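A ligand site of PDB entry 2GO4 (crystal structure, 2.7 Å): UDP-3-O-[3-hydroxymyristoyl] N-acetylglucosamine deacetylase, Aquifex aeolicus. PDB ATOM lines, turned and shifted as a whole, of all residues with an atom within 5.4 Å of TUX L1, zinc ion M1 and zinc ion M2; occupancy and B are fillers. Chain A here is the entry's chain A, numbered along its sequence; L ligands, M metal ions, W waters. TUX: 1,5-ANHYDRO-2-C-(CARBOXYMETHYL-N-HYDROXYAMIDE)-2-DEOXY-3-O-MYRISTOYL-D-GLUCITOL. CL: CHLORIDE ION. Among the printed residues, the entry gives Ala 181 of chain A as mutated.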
ATOM      1  N   ILE A  18      16.398  -6.294 -20.320  1.00  0.00           N
ATOM      2  CA  ILE A  18      16.706  -7.666 -20.705  1.00  0.00           C
ATOM      3  C   ILE A  18      15.649  -8.714 -20.331  1.00  0.00           C
ATOM      4  O   ILE A  18      15.498  -9.724 -21.024  1.00  0.00           O
ATOM      5  CB  ILE A  18      18.092  -8.097 -20.140  1.00  0.00           C
ATOM      6  CG1 ILE A  18      18.525  -9.388 -20.838  1.00  0.00           C
ATOM      7  CG2 ILE A  18      18.029  -8.282 -18.608  1.00  0.00           C
ATOM      8  CD1 ILE A  18      19.992  -9.725 -20.660  1.00  0.00           C
ATOM      9  N   HIS A  19      14.902  -8.491 -19.265  1.00  0.00           N
ATOM     10  CA  HIS A  19      13.901  -9.466 -18.871  1.00  0.00           C
ATOM     11  C   HIS A  19      12.485  -9.181 -19.352  1.00  0.00           C
ATOM     12  O   HIS A  19      11.779 -10.087 -19.785  1.00  0.00           O
ATOM     13  CB  HIS A  19      13.895  -9.648 -17.357  1.00  0.00           C
ATOM     14  CG  HIS A  19      15.102 -10.343 -16.822  1.00  0.00           C
ATOM     15  ND1 HIS A  19      15.558 -11.542 -17.339  1.00  0.00           N
ATOM     16  CD2 HIS A  19      15.940 -10.039 -15.805  1.00  0.00           C
ATOM     17  CE1 HIS A  19      16.618 -11.940 -16.659  1.00  0.00           C
ATOM     18  NE2 HIS A  19      16.877 -11.048 -15.723  1.00  0.00           N
ATOM     19  N   ASN A  57      16.267 -13.798  -8.607  1.00  0.00           N
ATOM     20  CA  ASN A  57      16.506 -14.837  -9.596  1.00  0.00           C
ATOM     21  C   ASN A  57      16.784 -14.184 -10.942  1.00  0.00           C
ATOM     22  O   ASN A  57      15.907 -13.533 -11.512  1.00  0.00           O
ATOM     23  CB  ASN A  57      15.286 -15.751  -9.754  1.00  0.00           C
ATOM     24  CG  ASN A  57      14.945 -16.502  -8.485  1.00  0.00           C
ATOM     25  OD1 ASN A  57      13.950 -17.219  -8.445  1.00  0.00           O
ATOM     26  ND2 ASN A  57      15.777 -16.336  -7.451  1.00  0.00           N
ATOM     27  N   HIS A  58      18.000 -14.348 -11.449  1.00  0.00           N
ATOM     28  CA  HIS A  58      18.370 -13.787 -12.748  1.00  0.00           C
ATOM     29  C   HIS A  58      18.526 -12.279 -12.767  1.00  0.00           C
ATOM     30  O   HIS A  58      18.826 -11.697 -13.803  1.00  0.00           O
ATOM     31  CB  HIS A  58      17.348 -14.212 -13.807  1.00  0.00           C
ATOM     32  CG  HIS A  58      17.145 -15.695 -13.865  1.00  0.00           C
ATOM     33  ND1 HIS A  58      18.147 -16.562 -14.268  1.00  0.00           N
ATOM     34  CD2 HIS A  58      16.089 -16.463 -13.521  1.00  0.00           C
ATOM     35  CE1 HIS A  58      17.712 -17.805 -14.151  1.00  0.00           C
ATOM     36  NE2 HIS A  58      16.468 -17.774 -13.702  1.00  0.00           N
ATOM     37  N   SER A  59      18.312 -11.651 -11.620  1.00  0.00           N
ATOM     38  CA  SER A  59      18.452 -10.203 -11.511  1.00  0.00           C
ATOM     39  C   SER A  59      18.050  -9.807 -10.125  1.00  0.00           C
ATOM     40  O   SER A  59      17.476 -10.600  -9.396  1.00  0.00           O
ATOM     41  CB  SER A  59      17.551  -9.469 -12.503  1.00  0.00           C
ATOM     42  OG  SER A  59      16.184  -9.503 -12.127  1.00  0.00           O
ATOM     43  N   GLU A  73      20.941  -3.924 -10.368  1.00  0.00           N
ATOM     44  CA  GLU A  73      22.346  -4.236 -10.110  1.00  0.00           C
ATOM     45  C   GLU A  73      23.411  -3.580 -10.970  1.00  0.00           C
ATOM     46  O   GLU A  73      24.445  -3.171 -10.444  1.00  0.00           O
ATOM     47  CB  GLU A  73      22.547  -5.755 -10.127  1.00  0.00           C
ATOM     48  CG  GLU A  73      22.318  -6.380 -11.485  1.00  0.00           C
ATOM     49  CD  GLU A  73      20.995  -7.101 -11.582  1.00  0.00           C
ATOM     50  OE1 GLU A  73      20.029  -6.682 -10.903  1.00  0.00           O
ATOM     51  OE2 GLU A  73      20.924  -8.090 -12.351  1.00  0.00           O
ATOM     52  N   HIS A  74      23.214  -3.463 -12.264  1.00  0.00           N
ATOM     53  CA  HIS A  74      24.256  -2.877 -13.087  1.00  0.00           C
ATOM     54  C   HIS A  74      24.445  -1.362 -12.872  1.00  0.00           C
ATOM     55  O   HIS A  74      25.565  -0.862 -12.818  1.00  0.00           O
ATOM     56  CB  HIS A  74      24.018  -3.198 -14.557  1.00  0.00           C
ATOM     57  CG  HIS A  74      24.023  -4.671 -14.842  1.00  0.00           C
ATOM     58  ND1 HIS A  74      23.848  -5.185 -16.117  1.00  0.00           N
ATOM     59  CD2 HIS A  74      24.159  -5.736 -14.028  1.00  0.00           C
ATOM     60  CE1 HIS A  74      23.884  -6.501 -16.057  1.00  0.00           C
ATOM     61  NE2 HIS A  74      24.069  -6.867 -14.807  1.00  0.00           N
ATOM     62  N   GLY A 101      24.669  -4.826 -21.857  1.00  0.00           N
ATOM     63  CA  GLY A 101      24.829  -5.933 -20.932  1.00  0.00           C
ATOM     64  C   GLY A 101      25.865  -5.698 -19.844  1.00  0.00           C
ATOM     65  O   GLY A 101      25.921  -6.470 -18.877  1.00  0.00           O
ATOM     66  N   THR A 179      26.707  -9.293 -19.379  1.00  0.00           N
ATOM     67  CA  THR A 179      25.834 -10.321 -18.825  1.00  0.00           C
ATOM     68  C   THR A 179      26.004 -11.560 -19.699  1.00  0.00           C
ATOM     69  O   THR A 179      26.035 -11.480 -20.932  1.00  0.00           O
ATOM     70  CB  THR A 179      24.376  -9.879 -18.907  1.00  0.00           C
ATOM     71  OG1 THR A 179      24.198  -8.714 -18.109  1.00  0.00           O
ATOM     72  CG2 THR A 179      23.449 -10.973 -18.449  1.00  0.00           C
ATOM     73  N   PHE A 180      26.081 -12.724 -19.071  1.00  0.00           N
ATOM     74  CA  PHE A 180      26.251 -13.940 -19.847  1.00  0.00           C
ATOM     75  C   PHE A 180      25.257 -15.009 -19.400  1.00  0.00           C
ATOM     76  O   PHE A 180      24.774 -15.009 -18.266  1.00  0.00           O
ATOM     77  CB  PHE A 180      27.681 -14.447 -19.664  1.00  0.00           C
ATOM     78  CG  PHE A 180      27.947 -14.972 -18.301  1.00  0.00           C
ATOM     79  CD1 PHE A 180      27.711 -16.309 -17.989  1.00  0.00           C
ATOM     80  CD2 PHE A 180      28.371 -14.106 -17.289  1.00  0.00           C
ATOM     81  CE1 PHE A 180      27.891 -16.784 -16.700  1.00  0.00           C
ATOM     82  CE2 PHE A 180      28.554 -14.562 -15.989  1.00  0.00           C
ATOM     83  CZ  PHE A 180      28.311 -15.905 -15.691  1.00  0.00           C
ATOM     84  N   ALA A 181      24.968 -15.936 -20.303  1.00  0.00           N
ATOM     85  CA  ALA A 181      24.058 -17.042 -20.013  1.00  0.00           C
ATOM     86  C   ALA A 181      24.490 -18.221 -20.861  1.00  0.00           C
ATOM     87  O   ALA A 181      25.150 -18.051 -21.894  1.00  0.00           O
ATOM     88  CB  ALA A 181      22.612 -16.666 -20.327  1.00  0.00           C
ATOM     89  N   ASP A 183      23.509 -21.566 -23.179  1.00  0.00           N
ATOM     90  CA  ASP A 183      22.424 -21.974 -24.069  1.00  0.00           C
ATOM     91  C   ASP A 183      21.406 -22.857 -23.358  1.00  0.00           C
ATOM     92  O   ASP A 183      20.196 -22.767 -23.624  1.00  0.00           O
ATOM     93  CB  ASP A 183      22.961 -22.668 -25.330  1.00  0.00           C
ATOM     94  CG  ASP A 183      24.012 -23.720 -25.029  1.00  0.00           C
ATOM     95  OD1 ASP A 183      24.035 -24.249 -23.906  1.00  0.00           O
ATOM     96  OD2 ASP A 183      24.799 -24.038 -25.939  1.00  0.00           O
ATOM     97  N   GLU A 185      20.459 -22.710 -20.257  1.00  0.00           N
ATOM     98  CA  GLU A 185      19.659 -21.895 -19.331  1.00  0.00           C
ATOM     99  C   GLU A 185      18.473 -21.224 -20.030  1.00  0.00           C
ATOM    100  O   GLU A 185      17.369 -21.138 -19.479  1.00  0.00           O
ATOM    101  CB  GLU A 185      20.505 -20.768 -18.750  1.00  0.00           C
ATOM    102  CG  GLU A 185      21.464 -21.086 -17.638  1.00  0.00           C
ATOM    103  CD  GLU A 185      21.969 -19.795 -16.991  1.00  0.00           C
ATOM    104  OE1 GLU A 185      22.602 -18.974 -17.695  1.00  0.00           O
ATOM    105  OE2 GLU A 185      21.705 -19.583 -15.784  1.00  0.00           O
ATOM    106  N   ILE A 186      18.730 -20.738 -21.232  1.00  0.00           N
ATOM    107  CA  ILE A 186      17.757 -20.008 -22.027  1.00  0.00           C
ATOM    108  C   ILE A 186      16.314 -20.517 -22.082  1.00  0.00           C
ATOM    109  O   ILE A 186      15.376 -19.754 -21.830  1.00  0.00           O
ATOM    110  CB  ILE A 186      18.300 -19.830 -23.453  1.00  0.00           C
ATOM    111  CG1 ILE A 186      19.615 -19.060 -23.396  1.00  0.00           C
ATOM    112  CG2 ILE A 186      17.289 -19.078 -24.321  1.00  0.00           C
ATOM    113  CD1 ILE A 186      20.266 -18.834 -24.733  1.00  0.00           C
ATOM    114  N   HIS A 188      14.787 -22.260 -20.094  1.00  0.00           N
ATOM    115  CA  HIS A 188      14.241 -22.106 -18.768  1.00  0.00           C
ATOM    116  C   HIS A 188      13.903 -20.659 -18.478  1.00  0.00           C
ATOM    117  O   HIS A 188      12.799 -20.336 -18.041  1.00  0.00           O
ATOM    118  CB  HIS A 188      15.246 -22.572 -17.735  1.00  0.00           C
ATOM    119  CG  HIS A 188      15.058 -21.941 -16.390  1.00  0.00           C
ATOM    120  ND1 HIS A 188      14.002 -22.253 -15.570  1.00  0.00           N
ATOM    121  CD2 HIS A 188      15.782 -21.000 -15.741  1.00  0.00           C
ATOM    122  CE1 HIS A 188      14.075 -21.524 -14.464  1.00  0.00           C
ATOM    123  NE2 HIS A 188      15.148 -20.756 -14.549  1.00  0.00           N
ATOM    124  N   ILE A 189      14.862 -19.780 -18.720  1.00  0.00           N
ATOM    125  CA  ILE A 189      14.644 -18.362 -18.484  1.00  0.00           C
ATOM    126  C   ILE A 189      13.427 -17.896 -19.271  1.00  0.00           C
ATOM    127  O   ILE A 189      12.605 -17.150 -18.757  1.00  0.00           O
ATOM    128  CB  ILE A 189      15.891 -17.532 -18.878  1.00  0.00           C
ATOM    129  CG1 ILE A 189      17.021 -17.837 -17.888  1.00  0.00           C
ATOM    130  CG2 ILE A 189      15.570 -16.053 -18.868  1.00  0.00           C
ATOM    131  CD1 ILE A 189      18.336 -17.226 -18.270  1.00  0.00           C
ATOM    132  N   LYS A 190      13.322 -18.353 -20.519  1.00  0.00           N
ATOM    133  CA  LYS A 190      12.172 -17.971 -21.348  1.00  0.00           C
ATOM    134  C   LYS A 190      10.864 -18.508 -20.769  1.00  0.00           C
ATOM    135  O   LYS A 190       9.836 -17.824 -20.794  1.00  0.00           O
ATOM    136  CB  LYS A 190      12.372 -18.470 -22.774  1.00  0.00           C
ATOM    137  CG  LYS A 190      13.348 -17.646 -23.597  1.00  0.00           C
ATOM    138  CD  LYS A 190      12.740 -16.303 -23.949  1.00  0.00           C
ATOM    139  CE  LYS A 190      13.594 -15.554 -24.955  1.00  0.00           C
ATOM    140  NZ  LYS A 190      12.865 -14.362 -25.483  1.00  0.00           N
ATOM    141  N   VAL A 192      10.029 -19.164 -17.564  1.00  0.00           N
ATOM    142  CA  VAL A 192       9.618 -18.470 -16.345  1.00  0.00           C
ATOM    143  C   VAL A 192       9.288 -16.989 -16.537  1.00  0.00           C
ATOM    144  O   VAL A 192       9.168 -16.249 -15.563  1.00  0.00           O
ATOM    145  CB  VAL A 192      10.703 -18.596 -15.254  1.00  0.00           C
ATOM    146  CG1 VAL A 192      10.934 -20.063 -14.943  1.00  0.00           C
ATOM    147  CG2 VAL A 192      12.004 -17.950 -15.723  1.00  0.00           C
ATOM    148  N   LEU A 194      11.155 -14.627 -18.248  1.00  0.00           N
ATOM    149  CA  LEU A 194      12.270 -13.691 -18.248  1.00  0.00           C
ATOM    150  C   LEU A 194      12.982 -13.638 -19.590  1.00  0.00           C
ATOM    151  O   LEU A 194      12.495 -14.172 -20.576  1.00  0.00           O
ATOM    152  CB  LEU A 194      13.233 -14.066 -17.119  1.00  0.00           C
ATOM    153  CG  LEU A 194      12.574 -14.111 -15.732  1.00  0.00           C
ATOM    154  CD1 LEU A 194      13.598 -14.489 -14.685  1.00  0.00           C
ATOM    155  CD2 LEU A 194      11.972 -12.752 -15.412  1.00  0.00           C
ATOM    156  N   GLY A 195      14.122 -12.955 -19.616  1.00  0.00           N
ATOM    157  CA  GLY A 195      14.916 -12.839 -20.827  1.00  0.00           C
ATOM    158  C   GLY A 195      14.182 -12.407 -22.087  1.00  0.00           C
ATOM    159  O   GLY A 195      14.702 -12.596 -23.192  1.00  0.00           O
ATOM    160  N   GLY A 198      16.399 -10.271 -24.230  1.00  0.00           N
ATOM    161  CA  GLY A 198      17.780 -10.688 -24.437  1.00  0.00           C
ATOM    162  C   GLY A 198      18.158 -11.083 -25.845  1.00  0.00           C
ATOM    163  O   GLY A 198      17.451 -11.802 -26.533  1.00  0.00           O
ATOM    164  N   SER A 199      19.319 -10.614 -26.277  1.00  0.00           N
ATOM    165  CA  SER A 199      19.823 -10.934 -27.611  1.00  0.00           C
ATOM    166  C   SER A 199      21.327 -11.084 -27.517  1.00  0.00           C
ATOM    167  O   SER A 199      21.888 -11.038 -26.421  1.00  0.00           O
ATOM    168  CB  SER A 199      19.465  -9.814 -28.582  1.00  0.00           C
ATOM    169  OG  SER A 199      20.147  -8.623 -28.245  1.00  0.00           O
ATOM    170  N   LEU A 200      21.986 -11.279 -28.646  1.00  0.00           N
ATOM    171  CA  LEU A 200      23.427 -11.409 -28.626  1.00  0.00           C
ATOM    172  C   LEU A 200      24.037 -10.016 -28.532  1.00  0.00           C
ATOM    173  O   LEU A 200      25.255  -9.867 -28.444  1.00  0.00           O
ATOM    174  CB  LEU A 200      23.928 -12.110 -29.892  1.00  0.00           C
ATOM    175  CG  LEU A 200      23.498 -13.572 -30.076  1.00  0.00           C
ATOM    176  CD1 LEU A 200      24.223 -14.136 -31.295  1.00  0.00           C
ATOM    177  CD2 LEU A 200      23.833 -14.398 -28.849  1.00  0.00           C
ATOM    178  N   THR A 203      23.736  -9.811 -24.352  1.00  0.00           N
ATOM    179  CA  THR A 203      24.050 -11.012 -23.582  1.00  0.00           C
ATOM    180  C   THR A 203      25.137 -11.817 -24.281  1.00  0.00           C
ATOM    181  O   THR A 203      25.194 -11.886 -25.503  1.00  0.00           O
ATOM    182  CB  THR A 203      22.794 -11.921 -23.439  1.00  0.00           C
ATOM    183  OG1 THR A 203      21.688 -11.142 -22.945  1.00  0.00           O
ATOM    184  CG2 THR A 203      23.081 -13.078 -22.475  1.00  0.00           C
ATOM    185  N   VAL A 205      26.246 -15.376 -24.940  1.00  0.00           N
ATOM    186  CA  VAL A 205      25.763 -16.750 -24.835  1.00  0.00           C
ATOM    187  C   VAL A 205      26.874 -17.755 -25.016  1.00  0.00           C
ATOM    188  O   VAL A 205      27.648 -17.710 -25.977  1.00  0.00           O
ATOM    189  CB  VAL A 205      24.624 -17.029 -25.846  1.00  0.00           C
ATOM    190  CG1 VAL A 205      23.924 -18.338 -25.481  1.00  0.00           C
ATOM    191  CG2 VAL A 205      23.633 -15.868 -25.853  1.00  0.00           C
ATOM    192  N   TYR A 212      28.572 -18.275 -28.776  1.00  0.00           N
ATOM    193  CA  TYR A 212      27.674 -17.887 -29.854  1.00  0.00           C
ATOM    194  C   TYR A 212      27.943 -16.507 -30.396  1.00  0.00           C
ATOM    195  O   TYR A 212      27.880 -16.308 -31.602  1.00  0.00           O
ATOM    196  CB  TYR A 212      26.221 -17.972 -29.393  1.00  0.00           C
ATOM    197  CG  TYR A 212      25.756 -19.377 -29.157  1.00  0.00           C
ATOM    198  CD1 TYR A 212      26.085 -20.056 -27.986  1.00  0.00           C
ATOM    199  CD2 TYR A 212      24.971 -20.040 -30.104  1.00  0.00           C
ATOM    200  CE1 TYR A 212      25.658 -21.356 -27.763  1.00  0.00           C
ATOM    201  CE2 TYR A 212      24.532 -21.346 -29.885  1.00  0.00           C
ATOM    202  CZ  TYR A 212      24.879 -21.988 -28.720  1.00  0.00           C
ATOM    203  OH  TYR A 212      24.442 -23.264 -28.480  1.00  0.00           O
ATOM    204  N   HIS A 226      32.164 -10.265 -14.617  1.00  0.00           N
ATOM    205  CA  HIS A 226      30.800  -9.756 -14.540  1.00  0.00           C
ATOM    206  C   HIS A 226      30.155 -10.131 -13.223  1.00  0.00           C
ATOM    207  O   HIS A 226      29.354  -9.385 -12.677  1.00  0.00           O
ATOM    208  CB  HIS A 226      29.943 -10.277 -15.682  1.00  0.00           C
ATOM    209  CG  HIS A 226      28.568  -9.679 -15.703  1.00  0.00           C
ATOM    210  ND1 HIS A 226      28.318  -8.421 -16.207  1.00  0.00           N
ATOM    211  CD2 HIS A 226      27.402 -10.122 -15.188  1.00  0.00           C
ATOM    212  CE1 HIS A 226      27.054  -8.112 -15.995  1.00  0.00           C
ATOM    213  NE2 HIS A 226      26.470  -9.124 -15.388  1.00  0.00           N
ATOM    214  N   LYS A 227      30.499 -11.306 -12.715  1.00  0.00           N
ATOM    215  CA  LYS A 227      29.956 -11.737 -11.437  1.00  0.00           C
ATOM    216  C   LYS A 227      30.466 -10.816 -10.334  1.00  0.00           C
ATOM    217  O   LYS A 227      29.765 -10.557  -9.360  1.00  0.00           O
ATOM    218  CB  LYS A 227      30.341 -13.181 -11.179  1.00  0.00           C
ATOM    219  CG  LYS A 227      29.521 -14.169 -11.966  1.00  0.00           C
ATOM    220  CD  LYS A 227      28.133 -14.313 -11.372  1.00  0.00           C
ATOM    221  CE  LYS A 227      27.223 -15.116 -12.278  1.00  0.00           C
ATOM    222  NZ  LYS A 227      25.903 -15.346 -11.627  1.00  0.00           N
ATOM    223  N   PHE A 229      31.281  -7.647 -10.870  1.00  0.00           N
ATOM    224  CA  PHE A 229      30.508  -6.453 -11.155  1.00  0.00           C
ATOM    225  C   PHE A 229      29.099  -6.582 -10.528  1.00  0.00           C
ATOM    226  O   PHE A 229      28.603  -5.634  -9.924  1.00  0.00           O
ATOM    227  CB  PHE A 229      30.388  -6.288 -12.670  1.00  0.00           C
ATOM    228  CG  PHE A 229      29.606  -5.086 -13.102  1.00  0.00           C
ATOM    229  CD1 PHE A 229      30.157  -3.798 -13.028  1.00  0.00           C
ATOM    230  CD2 PHE A 229      28.328  -5.224 -13.624  1.00  0.00           C
ATOM    231  CE1 PHE A 229      29.438  -2.683 -13.470  1.00  0.00           C
ATOM    232  CE2 PHE A 229      27.597  -4.115 -14.071  1.00  0.00           C
ATOM    233  CZ  PHE A 229      28.157  -2.830 -13.993  1.00  0.00           C
ATOM    234  N   ASP A 230      28.465  -7.747 -10.670  1.00  0.00           N
ATOM    235  CA  ASP A 230      27.133  -7.921 -10.094  1.00  0.00           C
ATOM    236  C   ASP A 230      27.170  -7.830  -8.578  1.00  0.00           C
ATOM    237  O   ASP A 230      26.307  -7.205  -7.986  1.00  0.00           O
ATOM    238  CB  ASP A 230      26.508  -9.282 -10.450  1.00  0.00           C
ATOM    239  CG  ASP A 230      25.937  -9.335 -11.857  1.00  0.00           C
ATOM    240  OD1 ASP A 230      25.549  -8.280 -12.398  1.00  0.00           O
ATOM    241  OD2 ASP A 230      25.851 -10.448 -12.404  1.00  0.00           O
ATOM    242  N   HIS A 253      22.981 -13.455  -7.080  1.00  0.00           N
ATOM    243  CA  HIS A 253      22.172 -12.413  -6.458  1.00  0.00           C
ATOM    244  C   HIS A 253      21.527 -12.843  -5.138  1.00  0.00           C
ATOM    245  O   HIS A 253      21.639 -12.139  -4.135  1.00  0.00           O
ATOM    246  CB  HIS A 253      21.101 -11.928  -7.435  1.00  0.00           C
ATOM    247  CG  HIS A 253      21.643 -11.309  -8.671  1.00  0.00           C
ATOM    248  ND1 HIS A 253      22.460 -10.189  -8.652  1.00  0.00           N
ATOM    249  CD2 HIS A 253      21.475 -11.618  -9.978  1.00  0.00           C
ATOM    250  CE1 HIS A 253      22.767  -9.846  -9.888  1.00  0.00           C
ATOM    251  NE2 HIS A 253      22.191 -10.696 -10.717  1.00  0.00           N
HETATM  252  C3G TUX L   1      21.425 -14.288 -15.635  1.00  0.00           C
HETATM  253  C4G TUX L   1      21.854 -15.697 -15.239  1.00  0.00           C
HETATM  254  C5G TUX L   1      21.744 -15.863 -13.717  1.00  0.00           C
HETATM  255  C2G TUX L   1      22.275 -13.265 -14.881  1.00  0.00           C
HETATM  256  C1G TUX L   1      22.197 -13.538 -13.371  1.00  0.00           C
HETATM  257  O5G TUX L   1      22.597 -14.893 -13.090  1.00  0.00           O
HETATM  258  O3G TUX L   1      21.620 -14.100 -17.044  1.00  0.00           O
HETATM  259  O1A TUX L   1      19.396 -13.706 -17.126  1.00  0.00           O
HETATM  260  C1A TUX L   1      20.478 -13.770 -17.711  1.00  0.00           C
HETATM  261  C2A TUX L   1      20.578 -13.527 -19.221  1.00  0.00           C
HETATM  262  C3A TUX L   1      19.211 -13.497 -19.904  1.00  0.00           C
HETATM  263  C4A TUX L   1      19.362 -13.997 -21.352  1.00  0.00           C
HETATM  264  C5A TUX L   1      18.062 -13.874 -22.143  1.00  0.00           C
HETATM  265  C6A TUX L   1      18.022 -14.809 -23.351  1.00  0.00           C
HETATM  266  C7A TUX L   1      19.180 -14.614 -24.338  1.00  0.00           C
HETATM  267  C8A TUX L   1      18.938 -15.471 -25.576  1.00  0.00           C
HETATM  268  C9A TUX L   1      20.110 -15.433 -26.556  1.00  0.00           C
HETATM  269  CAA TUX L   1      19.731 -16.135 -27.866  1.00  0.00           C
HETATM  270  CBA TUX L   1      20.895 -16.210 -28.854  1.00  0.00           C
HETATM  271  CCA TUX L   1      21.874 -17.354 -28.557  1.00  0.00           C
HETATM  272  CDA TUX L   1      21.355 -18.734 -29.006  1.00  0.00           C
HETATM  273  CEA TUX L   1      20.164 -19.221 -28.181  1.00  0.00           C
HETATM  274  CZH TUX L   1      21.810 -11.848 -15.218  1.00  0.00           C
HETATM  275  CYH TUX L   1      22.799 -10.772 -14.756  1.00  0.00           C
HETATM  276  OYH TUX L   1      23.775 -10.475 -15.446  1.00  0.00           O
HETATM  277  NXH TUX L   1      22.516 -10.217 -13.580  1.00  0.00           N
HETATM  278  OXH TUX L   1      23.314  -9.221 -13.111  1.00  0.00           O
HETATM  279  O4G TUX L   1      21.007 -16.646 -15.887  1.00  0.00           O
HETATM  280  C6G TUX L   1      22.160 -17.278 -13.326  1.00  0.00           C
HETATM  281  O6G TUX L   1      21.914 -17.498 -11.939  1.00  0.00           O
HETATM  282 CL    CL L   2      16.360 -20.117 -11.640  1.00  0.00          CL
HETATM  283 ZN    ZN M   1      24.757  -8.785 -14.358  1.00  0.00          ZN
HETATM  284 ZN    ZN M   2      15.074 -19.196 -12.851  1.00  0.00          ZN
HETATM  285  O   HOH W   1      13.148 -18.377 -11.971  1.00  0.00           O
HETATM  286  O   HOH W   2      21.025 -15.082 -10.314  1.00  0.00           O
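The side-chain hydroxyl (OG1) of Thr 179 lies close to an oxygen (OYH) of TUX L1 (3.2 Å). The side-chain carboxylate of Glu 185 is in hydrogen-bond range of an oxygen (O4G) of TUX L1. O4G of TUX L1 sits at hydrogen-bond distance from ND1 of His 58 (3.3 Å). NE2 of His 253 is in hydrogen-bond range of NXH of TUX L1, 2.9 Å away. NXH of TUX L1 is in hydrogen-bond range of OE2 of Glu 73 (2.9 Å).
The backbone carbonyl oxygen of His 58 lies within hydrogen-bond range of a ring nitrogen (NE2) of His 19 (2.8 Å). O of Ile 18 is in hydrogen-bond range of N of Gly 198, 3.4 Å away. The backbone carbonyl oxygen of Gly 195 sits at hydrogen-bond distance from the side-chain amino group of Lys 190 (3.4 Å). O of Ser 199 lies close to OG1 of Thr 203, at 3.5 Å. The backbone NH of Leu 194 is in hydrogen-bond range of the backbone carbonyl oxygen of Ile 189 (3.0 Å). ND1 of His 19 sits at hydrogen-bond distance from N of Gly 195 (3.0 Å). N of Tyr 212 sits at hydrogen-bond distance from O of Val 205 (3.0 Å). The side-chain hydroxyl (OH) of Tyr 212 sits at hydrogen-bond distance from the side-chain carboxylate (OD2) of Asp 183 (2.7 Å).
Merely in contact with TUX L1: His 19 (3.3 Å), Leu 200 (3.5 Å), Ile 186 (3.5 Å), Phe 180 (3.5 Å), Val 205 (3.6 Å), Gly 195 (3.6 Å), Ile 189 (3.6 Å), Lys 227 (3.6 Å), Ala 181 (3.9 Å), Ile 18 (3.9 Å), Gly 198 (3.9 Å), Thr 203 (3.99 Å) and Tyr 212 (3.998 Å). Hydrophobic or aromatic side chains that line TUX L1: Ile 18, His 19, His 58, His 74, Ala 181, Ile 186, Ile 189, Leu 200, Val 205, Tyr 212, His 226 and His 253. Within 4 Å of TUX L1: Ile 18, His 19, His 58, Glu 73, His 74, Thr 179, Phe 180, Ala 181, Glu 185, Ile 186, Ile 189, Gly 195, Gly 198, Leu 200, Thr 203, Val 205, Tyr 212, His 226, Lys 227, Asp 230 and His 253. The nearest printed residue that does not touch TUX L1 is Ser 199 (4.4 Å).
Thr 179 touches zinc ion M1 (OG1 to ZN, 3.8 Å). Of the 31 residues printed, 4 come within 4 Å of zinc ion M1.
Of the 31 residues printed, 2 come within 4 Å of zinc ion M2.
Zinc ion M1 is bound by OXH of TUX L1 (2.0 Å), NE2 of His 226 (2.0 Å), NE2 of His 74 (2.1 Å), OD1 of Asp 230 (2.2 Å) and OYH of TUX L1 (2.2 Å). Zinc ion M1 has five donor atoms within binding distance. Slightly farther from zinc ion M1 lies the side-chain carboxylate (OD2) of Asp 230 (2.8 Å).
Zinc ion M2 is bound by CL of CL L2 (2.0 Å), NE2 of His 58 (2.2 Å), water W1 (2.3 Å) and NE2 of His 188 (2.3 Å). Zinc ion M2 has four donor atoms within binding distance.
Water W2 lies within hydrogen-bond range of an oxygen (O6G) of TUX L1 (3.0 Å) and the backbone NH of His 58 (3.3 Å).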
